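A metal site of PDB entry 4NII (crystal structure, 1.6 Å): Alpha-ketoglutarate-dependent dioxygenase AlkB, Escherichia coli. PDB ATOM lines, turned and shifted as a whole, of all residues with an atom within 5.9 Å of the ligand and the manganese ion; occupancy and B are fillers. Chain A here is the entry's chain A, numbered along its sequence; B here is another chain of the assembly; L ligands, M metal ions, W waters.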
ATOM      1  N   MET A  50      -8.498   3.633  -0.609  1.00  0.00           N
ATOM      2  CA  MET A  50      -8.647   3.117  -1.963  1.00  0.00           C
ATOM      3  C   MET A  50      -8.285   4.152  -3.034  1.00  0.00           C
ATOM      4  O   MET A  50      -8.402   5.386  -2.824  1.00  0.00           O
ATOM      5  CB  MET A  50     -10.081   2.668  -2.203  1.00  0.00           C
ATOM      6  CG  MET A  50     -10.388   1.477  -1.411  1.00  0.00           C
ATOM      7  SD  MET A  50     -12.137   1.016  -1.502  1.00  0.00           S
ATOM      8  CE  MET A  50     -12.144  -0.661  -0.895  1.00  0.00           C
ATOM      9  N   LEU A 107      -8.822  -1.853  -8.703  1.00  0.00           N
ATOM     10  CA  LEU A 107      -9.035  -1.176  -7.414  1.00  0.00           C
ATOM     11  C   LEU A 107      -7.852  -1.459  -6.557  1.00  0.00           C
ATOM     12  O   LEU A 107      -7.457  -2.611  -6.381  1.00  0.00           O
ATOM     13  CB  LEU A 107     -10.286  -1.687  -6.746  1.00  0.00           C
ATOM     14  CG  LEU A 107     -10.618  -1.304  -5.337  1.00  0.00           C
ATOM     15  CD1 LEU A 107     -10.959   0.162  -5.258  1.00  0.00           C
ATOM     16  CD2 LEU A 107     -11.804  -2.077  -4.788  1.00  0.00           C
ATOM     17  N   ASN A 109      -6.180  -1.085  -2.930  1.00  0.00           N
ATOM     18  CA  ASN A 109      -6.476  -0.979  -1.504  1.00  0.00           C
ATOM     19  C   ASN A 109      -5.195  -0.846  -0.669  1.00  0.00           C
ATOM     20  O   ASN A 109      -4.253  -1.600  -0.860  1.00  0.00           O
ATOM     21  CB  ASN A 109      -7.224  -2.246  -1.054  1.00  0.00           C
ATOM     22  CG  ASN A 109      -8.563  -2.440  -1.741  1.00  0.00           C
ATOM     23  OD1 ASN A 109      -8.873  -3.524  -2.233  1.00  0.00           O
ATOM     24  ND2 ASN A 109      -9.367  -1.428  -1.763  1.00  0.00           N
ATOM     25  N   TYR A 111      -4.094  -1.047   3.294  1.00  0.00           N
ATOM     26  CA  TYR A 111      -4.447  -1.403   4.662  1.00  0.00           C
ATOM     27  C   TYR A 111      -3.346  -0.925   5.607  1.00  0.00           C
ATOM     28  O   TYR A 111      -2.234  -1.379   5.532  1.00  0.00           O
ATOM     29  CB  TYR A 111      -4.538  -2.903   4.829  1.00  0.00           C
ATOM     30  CG  TYR A 111      -5.634  -3.541   3.997  1.00  0.00           C
ATOM     31  CD1 TYR A 111      -5.482  -3.748   2.627  1.00  0.00           C
ATOM     32  CD2 TYR A 111      -6.817  -3.934   4.588  1.00  0.00           C
ATOM     33  CE1 TYR A 111      -6.524  -4.342   1.886  1.00  0.00           C
ATOM     34  CE2 TYR A 111      -7.825  -4.568   3.866  1.00  0.00           C
ATOM     35  CZ  TYR A 111      -7.679  -4.710   2.509  1.00  0.00           C
ATOM     36  OH  TYR A 111      -8.694  -5.281   1.756  1.00  0.00           O
ATOM     37  N   LEU A 117     -11.738  -5.352   5.762  1.00  0.00           N
ATOM     38  CA  LEU A 117     -12.814  -5.283   4.811  1.00  0.00           C
ATOM     39  C   LEU A 117     -13.788  -6.381   5.147  1.00  0.00           C
ATOM     40  O   LEU A 117     -13.469  -7.560   4.959  1.00  0.00           O
ATOM     41  CB  LEU A 117     -12.252  -5.420   3.414  1.00  0.00           C
ATOM     42  CG  LEU A 117     -13.045  -4.975   2.223  1.00  0.00           C
ATOM     43  CD1 LEU A 117     -13.644  -3.591   2.342  1.00  0.00           C
ATOM     44  CD2 LEU A 117     -12.219  -5.088   0.931  1.00  0.00           C
ATOM     45  N   HIS A 120     -18.133  -9.471   1.948  1.00  0.00           N
ATOM     46  CA  HIS A 120     -18.917  -8.876   0.934  1.00  0.00           C
ATOM     47  C   HIS A 120     -18.751  -9.702  -0.325  1.00  0.00           C
ATOM     48  O   HIS A 120     -17.935 -10.623  -0.376  1.00  0.00           O
ATOM     49  CB  HIS A 120     -18.450  -7.448   0.691  1.00  0.00           C
ATOM     50  CG  HIS A 120     -17.092  -7.377   0.094  1.00  0.00           C
ATOM     51  ND1 HIS A 120     -15.941  -7.380   0.855  1.00  0.00           N
ATOM     52  CD2 HIS A 120     -16.681  -7.330  -1.200  1.00  0.00           C
ATOM     53  CE1 HIS A 120     -14.895  -7.365   0.058  1.00  0.00           C
ATOM     54  NE2 HIS A 120     -15.313  -7.263  -1.186  1.00  0.00           N
ATOM     55  N   GLN A 121     -19.606  -9.426  -1.306  1.00  0.00           N
ATOM     56  CA  GLN A 121     -19.534 -10.023  -2.637  1.00  0.00           C
ATOM     57  C   GLN A 121     -19.120  -8.969  -3.617  1.00  0.00           C
ATOM     58  O   GLN A 121     -19.490  -7.786  -3.460  1.00  0.00           O
ATOM     59  CB  GLN A 121     -20.886 -10.551  -3.054  1.00  0.00           C
ATOM     60  CG  GLN A 121     -21.466 -11.592  -2.140  1.00  0.00           C
ATOM     61  CD  GLN A 121     -22.899 -11.955  -2.560  1.00  0.00           C
ATOM     62  OE1 GLN A 121     -23.829 -11.168  -2.380  1.00  0.00           O
ATOM     63  NE2 GLN A 121     -23.049 -13.078  -3.197  1.00  0.00           N
ATOM     64  N   ASP A 122     -18.395  -9.368  -4.658  1.00  0.00           N
ATOM     65  CA  ASP A 122     -18.065  -8.445  -5.745  1.00  0.00           C
ATOM     66  C   ASP A 122     -19.158  -8.597  -6.806  1.00  0.00           C
ATOM     67  O   ASP A 122     -19.178  -9.566  -7.586  1.00  0.00           O
ATOM     68  CB  ASP A 122     -16.684  -8.694  -6.355  1.00  0.00           C
ATOM     69  CG  ASP A 122     -15.571  -8.086  -5.561  1.00  0.00           C
ATOM     70  OD1 ASP A 122     -15.700  -8.019  -4.325  1.00  0.00           O
ATOM     71  OD2 ASP A 122     -14.547  -7.656  -6.179  1.00  0.00           O
ATOM     72  N   SER A 134      -6.762 -10.959  -7.654  1.00  0.00           N
ATOM     73  CA  SER A 134      -6.510 -10.193  -6.427  1.00  0.00           C
ATOM     74  C   SER A 134      -5.078 -10.437  -5.952  1.00  0.00           C
ATOM     75  O   SER A 134      -4.732 -11.551  -5.580  1.00  0.00           O
ATOM     76  CB  SER A 134      -7.518 -10.648  -5.361  1.00  0.00           C
ATOM     77  OG  SER A 134      -7.479  -9.817  -4.230  1.00  0.00           O
ATOM     78  N   SER A 136      -1.754  -9.525  -3.527  1.00  0.00           N
ATOM     79  CA  SER A 136      -1.385  -9.049  -2.179  1.00  0.00           C
ATOM     80  C   SER A 136       0.055  -8.535  -2.224  1.00  0.00           C
ATOM     81  O   SER A 136       0.952  -9.220  -2.789  1.00  0.00           O
ATOM     82  CB  SER A 136      -1.415 -10.171  -1.147  1.00  0.00           C
ATOM     83  OG  SER A 136      -2.747 -10.646  -1.001  1.00  0.00           O
ATOM     84  N   PHE A 143      -7.364 -13.603   4.940  1.00  0.00           N
ATOM     85  CA  PHE A 143      -8.376 -13.472   3.925  1.00  0.00           C
ATOM     86  C   PHE A 143      -9.415 -14.492   4.282  1.00  0.00           C
ATOM     87  O   PHE A 143      -9.036 -15.597   4.569  1.00  0.00           O
ATOM     88  CB  PHE A 143      -7.762 -13.802   2.579  1.00  0.00           C
ATOM     89  CG  PHE A 143      -8.696 -13.754   1.422  1.00  0.00           C
ATOM     90  CD1 PHE A 143      -9.323 -12.571   1.033  1.00  0.00           C
ATOM     91  CD2 PHE A 143      -8.850 -14.864   0.602  1.00  0.00           C
ATOM     92  CE1 PHE A 143     -10.142 -12.536  -0.077  1.00  0.00           C
ATOM     93  CE2 PHE A 143      -9.652 -14.825  -0.550  1.00  0.00           C
ATOM     94  CZ  PHE A 143     -10.317 -13.667  -0.859  1.00  0.00           C
ATOM     95  N   LEU A 159      -2.657 -14.452   3.497  1.00  0.00           N
ATOM     96  CA  LEU A 159      -2.134 -13.988   2.219  1.00  0.00           C
ATOM     97  C   LEU A 159      -0.856 -13.193   2.496  1.00  0.00           C
ATOM     98  O   LEU A 159      -0.827 -12.221   3.277  1.00  0.00           O
ATOM     99  CB  LEU A 159      -3.142 -13.127   1.487  1.00  0.00           C
ATOM    100  CG  LEU A 159      -4.458 -13.811   1.133  1.00  0.00           C
ATOM    101  CD1 LEU A 159      -5.385 -12.885   0.353  1.00  0.00           C
ATOM    102  CD2 LEU A 159      -4.136 -15.035   0.305  1.00  0.00           C
ATOM    103  N   TRP A 167     -10.648 -15.834  -8.413  1.00  0.00           N
ATOM    104  CA  TRP A 167     -11.920 -16.524  -8.342  1.00  0.00           C
ATOM    105  C   TRP A 167     -12.832 -16.158  -9.491  1.00  0.00           C
ATOM    106  O   TRP A 167     -12.749 -15.076 -10.078  1.00  0.00           O
ATOM    107  CB  TRP A 167     -12.577 -16.446  -6.962  1.00  0.00           C
ATOM    108  CG  TRP A 167     -13.026 -15.131  -6.454  1.00  0.00           C
ATOM    109  CD1 TRP A 167     -14.304 -14.671  -6.372  1.00  0.00           C
ATOM    110  CD2 TRP A 167     -12.213 -14.167  -5.808  1.00  0.00           C
ATOM    111  NE1 TRP A 167     -14.347 -13.460  -5.740  1.00  0.00           N
ATOM    112  CE2 TRP A 167     -13.056 -13.110  -5.400  1.00  0.00           C
ATOM    113  CE3 TRP A 167     -10.854 -14.090  -5.523  1.00  0.00           C
ATOM    114  CZ2 TRP A 167     -12.575 -11.989  -4.737  1.00  0.00           C
ATOM    115  CZ3 TRP A 167     -10.372 -12.985  -4.887  1.00  0.00           C
ATOM    116  CH2 TRP A 167     -11.229 -11.943  -4.500  1.00  0.00           C
ATOM    117  N   HIS A 176     -16.311 -12.836   0.681  1.00  0.00           N
ATOM    118  CA  HIS A 176     -14.906 -12.818   1.068  1.00  0.00           C
ATOM    119  C   HIS A 176     -14.616 -11.501   1.792  1.00  0.00           C
ATOM    120  O   HIS A 176     -15.421 -10.546   1.773  1.00  0.00           O
ATOM    121  CB  HIS A 176     -14.021 -12.972  -0.159  1.00  0.00           C
ATOM    122  CG  HIS A 176     -14.247 -11.904  -1.165  1.00  0.00           C
ATOM    123  ND1 HIS A 176     -15.343 -11.894  -2.001  1.00  0.00           N
ATOM    124  CD2 HIS A 176     -13.594 -10.751  -1.397  1.00  0.00           C
ATOM    125  CE1 HIS A 176     -15.322 -10.799  -2.745  1.00  0.00           C
ATOM    126  NE2 HIS A 176     -14.259 -10.098  -2.408  1.00  0.00           N
ATOM    127  N   GLY A 177     -13.441 -11.445   2.416  1.00  0.00           N
ATOM    128  CA  GLY A 177     -13.118 -10.298   3.243  1.00  0.00           C
ATOM    129  C   GLY A 177     -11.722 -10.423   3.799  1.00  0.00           C
ATOM    130  O   GLY A 177     -11.052 -11.448   3.571  1.00  0.00           O
ATOM    131  N   ILE A 178     -11.330  -9.379   4.514  1.00  0.00           N
ATOM    132  CA  ILE A 178     -10.018  -9.263   5.159  1.00  0.00           C
ATOM    133  C   ILE A 178     -10.162  -8.890   6.628  1.00  0.00           C
ATOM    134  O   ILE A 178     -10.882  -7.943   6.992  1.00  0.00           O
ATOM    135  CB  ILE A 178      -9.137  -8.228   4.447  1.00  0.00           C
ATOM    136  CG1 ILE A 178      -8.782  -8.632   3.009  1.00  0.00           C
ATOM    137  CG2 ILE A 178      -7.877  -7.937   5.258  1.00  0.00           C
ATOM    138  CD1 ILE A 178      -7.785  -9.719   2.892  1.00  0.00           C
ATOM    139  N   ARG A 193      -0.218  -2.993   3.969  1.00  0.00           N
ATOM    140  CA  ARG A 193      -0.510  -3.977   2.937  1.00  0.00           C
ATOM    141  C   ARG A 193      -1.255  -3.279   1.794  1.00  0.00           C
ATOM    142  O   ARG A 193      -2.072  -2.379   2.018  1.00  0.00           O
ATOM    143  CB  ARG A 193      -1.390  -5.087   3.498  1.00  0.00           C
ATOM    144  CG  ARG A 193      -1.949  -6.045   2.451  1.00  0.00           C
ATOM    145  CD  ARG A 193      -2.720  -7.193   3.080  1.00  0.00           C
ATOM    146  NE  ARG A 193      -3.126  -8.166   2.060  1.00  0.00           N
ATOM    147  CZ  ARG A 193      -4.311  -8.177   1.457  1.00  0.00           C
ATOM    148  NH1 ARG A 193      -5.231  -7.267   1.744  1.00  0.00           N
ATOM    149  NH2 ARG A 193      -4.568  -9.110   0.540  1.00  0.00           N
ATOM    150  N   ASN A 195      -3.470  -4.261  -1.773  1.00  0.00           N
ATOM    151  CA  ASN A 195      -4.059  -5.250  -2.653  1.00  0.00           C
ATOM    152  C   ASN A 195      -4.461  -4.599  -3.977  1.00  0.00           C
ATOM    153  O   ASN A 195      -4.953  -3.493  -4.002  1.00  0.00           O
ATOM    154  CB  ASN A 195      -5.242  -5.885  -1.925  1.00  0.00           C
ATOM    155  CG  ASN A 195      -5.820  -7.050  -2.683  1.00  0.00           C
ATOM    156  OD1 ASN A 195      -6.791  -6.897  -3.369  1.00  0.00           O
ATOM    157  ND2 ASN A 195      -5.245  -8.206  -2.535  1.00  0.00           N
ATOM    158  N   THR A 197      -7.103  -5.364  -7.066  1.00  0.00           N
ATOM    159  CA  THR A 197      -8.284  -6.150  -7.475  1.00  0.00           C
ATOM    160  C   THR A 197      -8.616  -5.807  -8.918  1.00  0.00           C
ATOM    161  O   THR A 197      -9.024  -4.684  -9.201  1.00  0.00           O
ATOM    162  CB  THR A 197      -9.438  -5.813  -6.570  1.00  0.00           C
ATOM    163  OG1 THR A 197      -9.120  -6.290  -5.254  1.00  0.00           O
ATOM    164  CG2 THR A 197     -10.673  -6.569  -7.046  1.00  0.00           C
ATOM    165  P   6MA B   8     -21.470  -4.858   2.096  1.00  0.00           P
ATOM    166  OP1 6MA B   8     -21.844  -4.012   0.934  1.00  0.00           O
ATOM    167  OP2 6MA B   8     -21.184  -6.307   1.989  1.00  0.00           O
ATOM    168  O5' 6MA B   8     -20.053  -4.131   2.582  1.00  0.00           O
ATOM    169  C5' 6MA B   8     -19.192  -4.814   3.468  1.00  0.00           C
ATOM    170  C4' 6MA B   8     -17.835  -4.149   3.334  1.00  0.00           C
ATOM    171  O4' 6MA B   8     -17.356  -4.483   2.024  1.00  0.00           O
ATOM    172  C3' 6MA B   8     -17.928  -2.663   3.434  1.00  0.00           C
ATOM    173  O3' 6MA B   8     -16.669  -2.085   3.899  1.00  0.00           O
ATOM    174  C2' 6MA B   8     -18.064  -2.260   1.985  1.00  0.00           C
ATOM    175  C1' 6MA B   8     -17.176  -3.284   1.264  1.00  0.00           C
ATOM    176  N9  6MA B   8     -17.537  -3.559  -0.129  1.00  0.00           N
ATOM    177  C8  6MA B   8     -18.759  -4.007  -0.527  1.00  0.00           C
ATOM    178  N7  6MA B   8     -18.739  -4.240  -1.839  1.00  0.00           N
ATOM    179  C5  6MA B   8     -17.474  -4.043  -2.296  1.00  0.00           C
ATOM    180  C6  6MA B   8     -16.800  -4.178  -3.596  1.00  0.00           C
ATOM    181  N1  6MA B   8     -15.470  -3.909  -3.668  1.00  0.00           N
ATOM    182  C2  6MA B   8     -14.806  -3.553  -2.566  1.00  0.00           C
ATOM    183  N3  6MA B   8     -15.367  -3.396  -1.340  1.00  0.00           N
ATOM    184  C4  6MA B   8     -16.682  -3.643  -1.157  1.00  0.00           C
ATOM    185  N6  6MA B   8     -17.591  -4.543  -4.635  1.00  0.00           N
ATOM    186  C1  6MA B   8     -17.075  -4.559  -6.025  1.00  0.00           C
HETATM  187  C1  LIG L   1     -11.866  -5.824  -2.686  1.00  0.00           C
HETATM  188  O1  LIG L   1     -13.012  -5.990  -3.248  1.00  0.00           O
HETATM  189  O2  LIG L   1     -11.174  -4.768  -2.754  1.00  0.00           O
HETATM  190  C2  LIG L   1     -11.308  -6.926  -1.896  1.00  0.00           C
HETATM  191  O3  LIG L   1     -12.014  -7.879  -1.661  1.00  0.00           O
HETATM  192  C3  LIG L   1      -9.890  -6.847  -1.346  1.00  0.00           C
HETATM  193  C4  LIG L   1      -9.396  -8.196  -0.834  1.00  0.00           C
HETATM  194  C5  LIG L   1      -7.953  -8.113  -0.371  1.00  0.00           C
HETATM  195  O4  LIG L   1      -7.245  -9.132  -0.461  1.00  0.00           O
HETATM  196  O5  LIG L   1      -7.515  -7.054   0.121  1.00  0.00           O
HETATM  197 MN    MN M   1     -14.048  -7.909  -2.917  1.00  0.00          MN
HETATM  198  O   HOH W   1     -12.642  -8.687  -4.674  1.00  0.00           O
HETATM  199  O   HOH W   2     -10.174  -8.587  -4.227  1.00  0.00           O
HETATM  200  O   HOH W   3      -7.397 -11.355  -1.949  1.00  0.00           O
HETATM  201  O   HOH W   4     -13.774  -5.021  -5.443  1.00  0.00           O
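The side-chain amide oxygen (OD1) of Asn 109 lies close to an oxygen (O2) of the ligand.
The side-chain hydroxyl of Tyr 111 is in hydrogen-bond range of an oxygen (O5) of the ligand (2.7 Å).
NH1 of Arg 193 is in salt-bridge range of O5 of the ligand, at 2.8 Å.
O4 of the ligand lies within hydrogen-bond range of ND2 of Asn 195, at 3.0 Å.
A ring nitrogen (ND1) of His 120 sits at hydrogen-bond distance from O4' of 6MA 8 of chain B (3.4 Å).
ND2 of Asn 109 lies close to SD of Met 50 (3.7 Å).
The backbone carbonyl oxygen (O) of Arg 193 sits at hydrogen-bond distance from the backbone NH (N) of Tyr 111, at 2.7 Å.
The side-chain amide nitrogen of Asn 195 sits close to the guanidinium group of Arg 193, at 3.3 Å.
The side-chain hydroxyl (OG) of Ser 136 lies within hydrogen-bond range of the guanidinium group (NH2) of Arg 193 (2.8 Å).
The side-chain amide oxygen (OD1) of Asn 195 lies within hydrogen-bond range of the side-chain hydroxyl (OG1) of Thr 197, at 3.1 Å.
OD1 of Asn 195 sits at hydrogen-bond distance from OG of Ser 134 (3.1 Å).
The backbone NH (N) of Thr 197 is in hydrogen-bond range of the backbone carbonyl oxygen (O) of Leu 107 (2.9 Å).
N1 of 6MA 8 of chain B lies close to an oxygen (O1) of the ligand.
Merely in contact with the ligand: Leu 107 (3.4 Å), Ile 178 (3.4 Å), Leu 117 (3.5 Å), Thr 197 (3.6 Å) and Ser 134 (3.8 Å).
Hydrophobic or aromatic side chains within 4 Å of the ligand: Leu 107, Tyr 111, Leu 117, His 120, His 176 and Ile 178.
Along chain A the residues within 4 Å of the ligand span positions 107 to 197.
The nearest printed residue that does not touch the manganese ion is 6MA 8 of chain B (4.3 Å).
The manganese ion is bound by the side-chain carboxylate (OD1) of Asp 122 (2.2 Å), an oxygen (O1) of the ligand (2.2 Å), a ring nitrogen (NE2) of His 120 (2.2 Å), a ring nitrogen (NE2) of His 176 (2.3 Å), water W1 (2.4 Å) and an oxygen (O3) of the ligand (2.4 Å).
The manganese ion has six donor atoms within binding distance.
Water W4 bridges N1 of 6MA 8 of chain B (2.7 Å) and OD2 of Asp 122 (2.8 Å).
Water W3 lies within hydrogen-bond range of O4 of the ligand (2.7 Å) and OG of Ser 134 (2.8 Å).
Water W2 bridges the side-chain hydroxyl (OG1) of Thr 197 (2.7 Å) and the side-chain hydroxyl (OG) of Ser 134 (3.0 Å).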
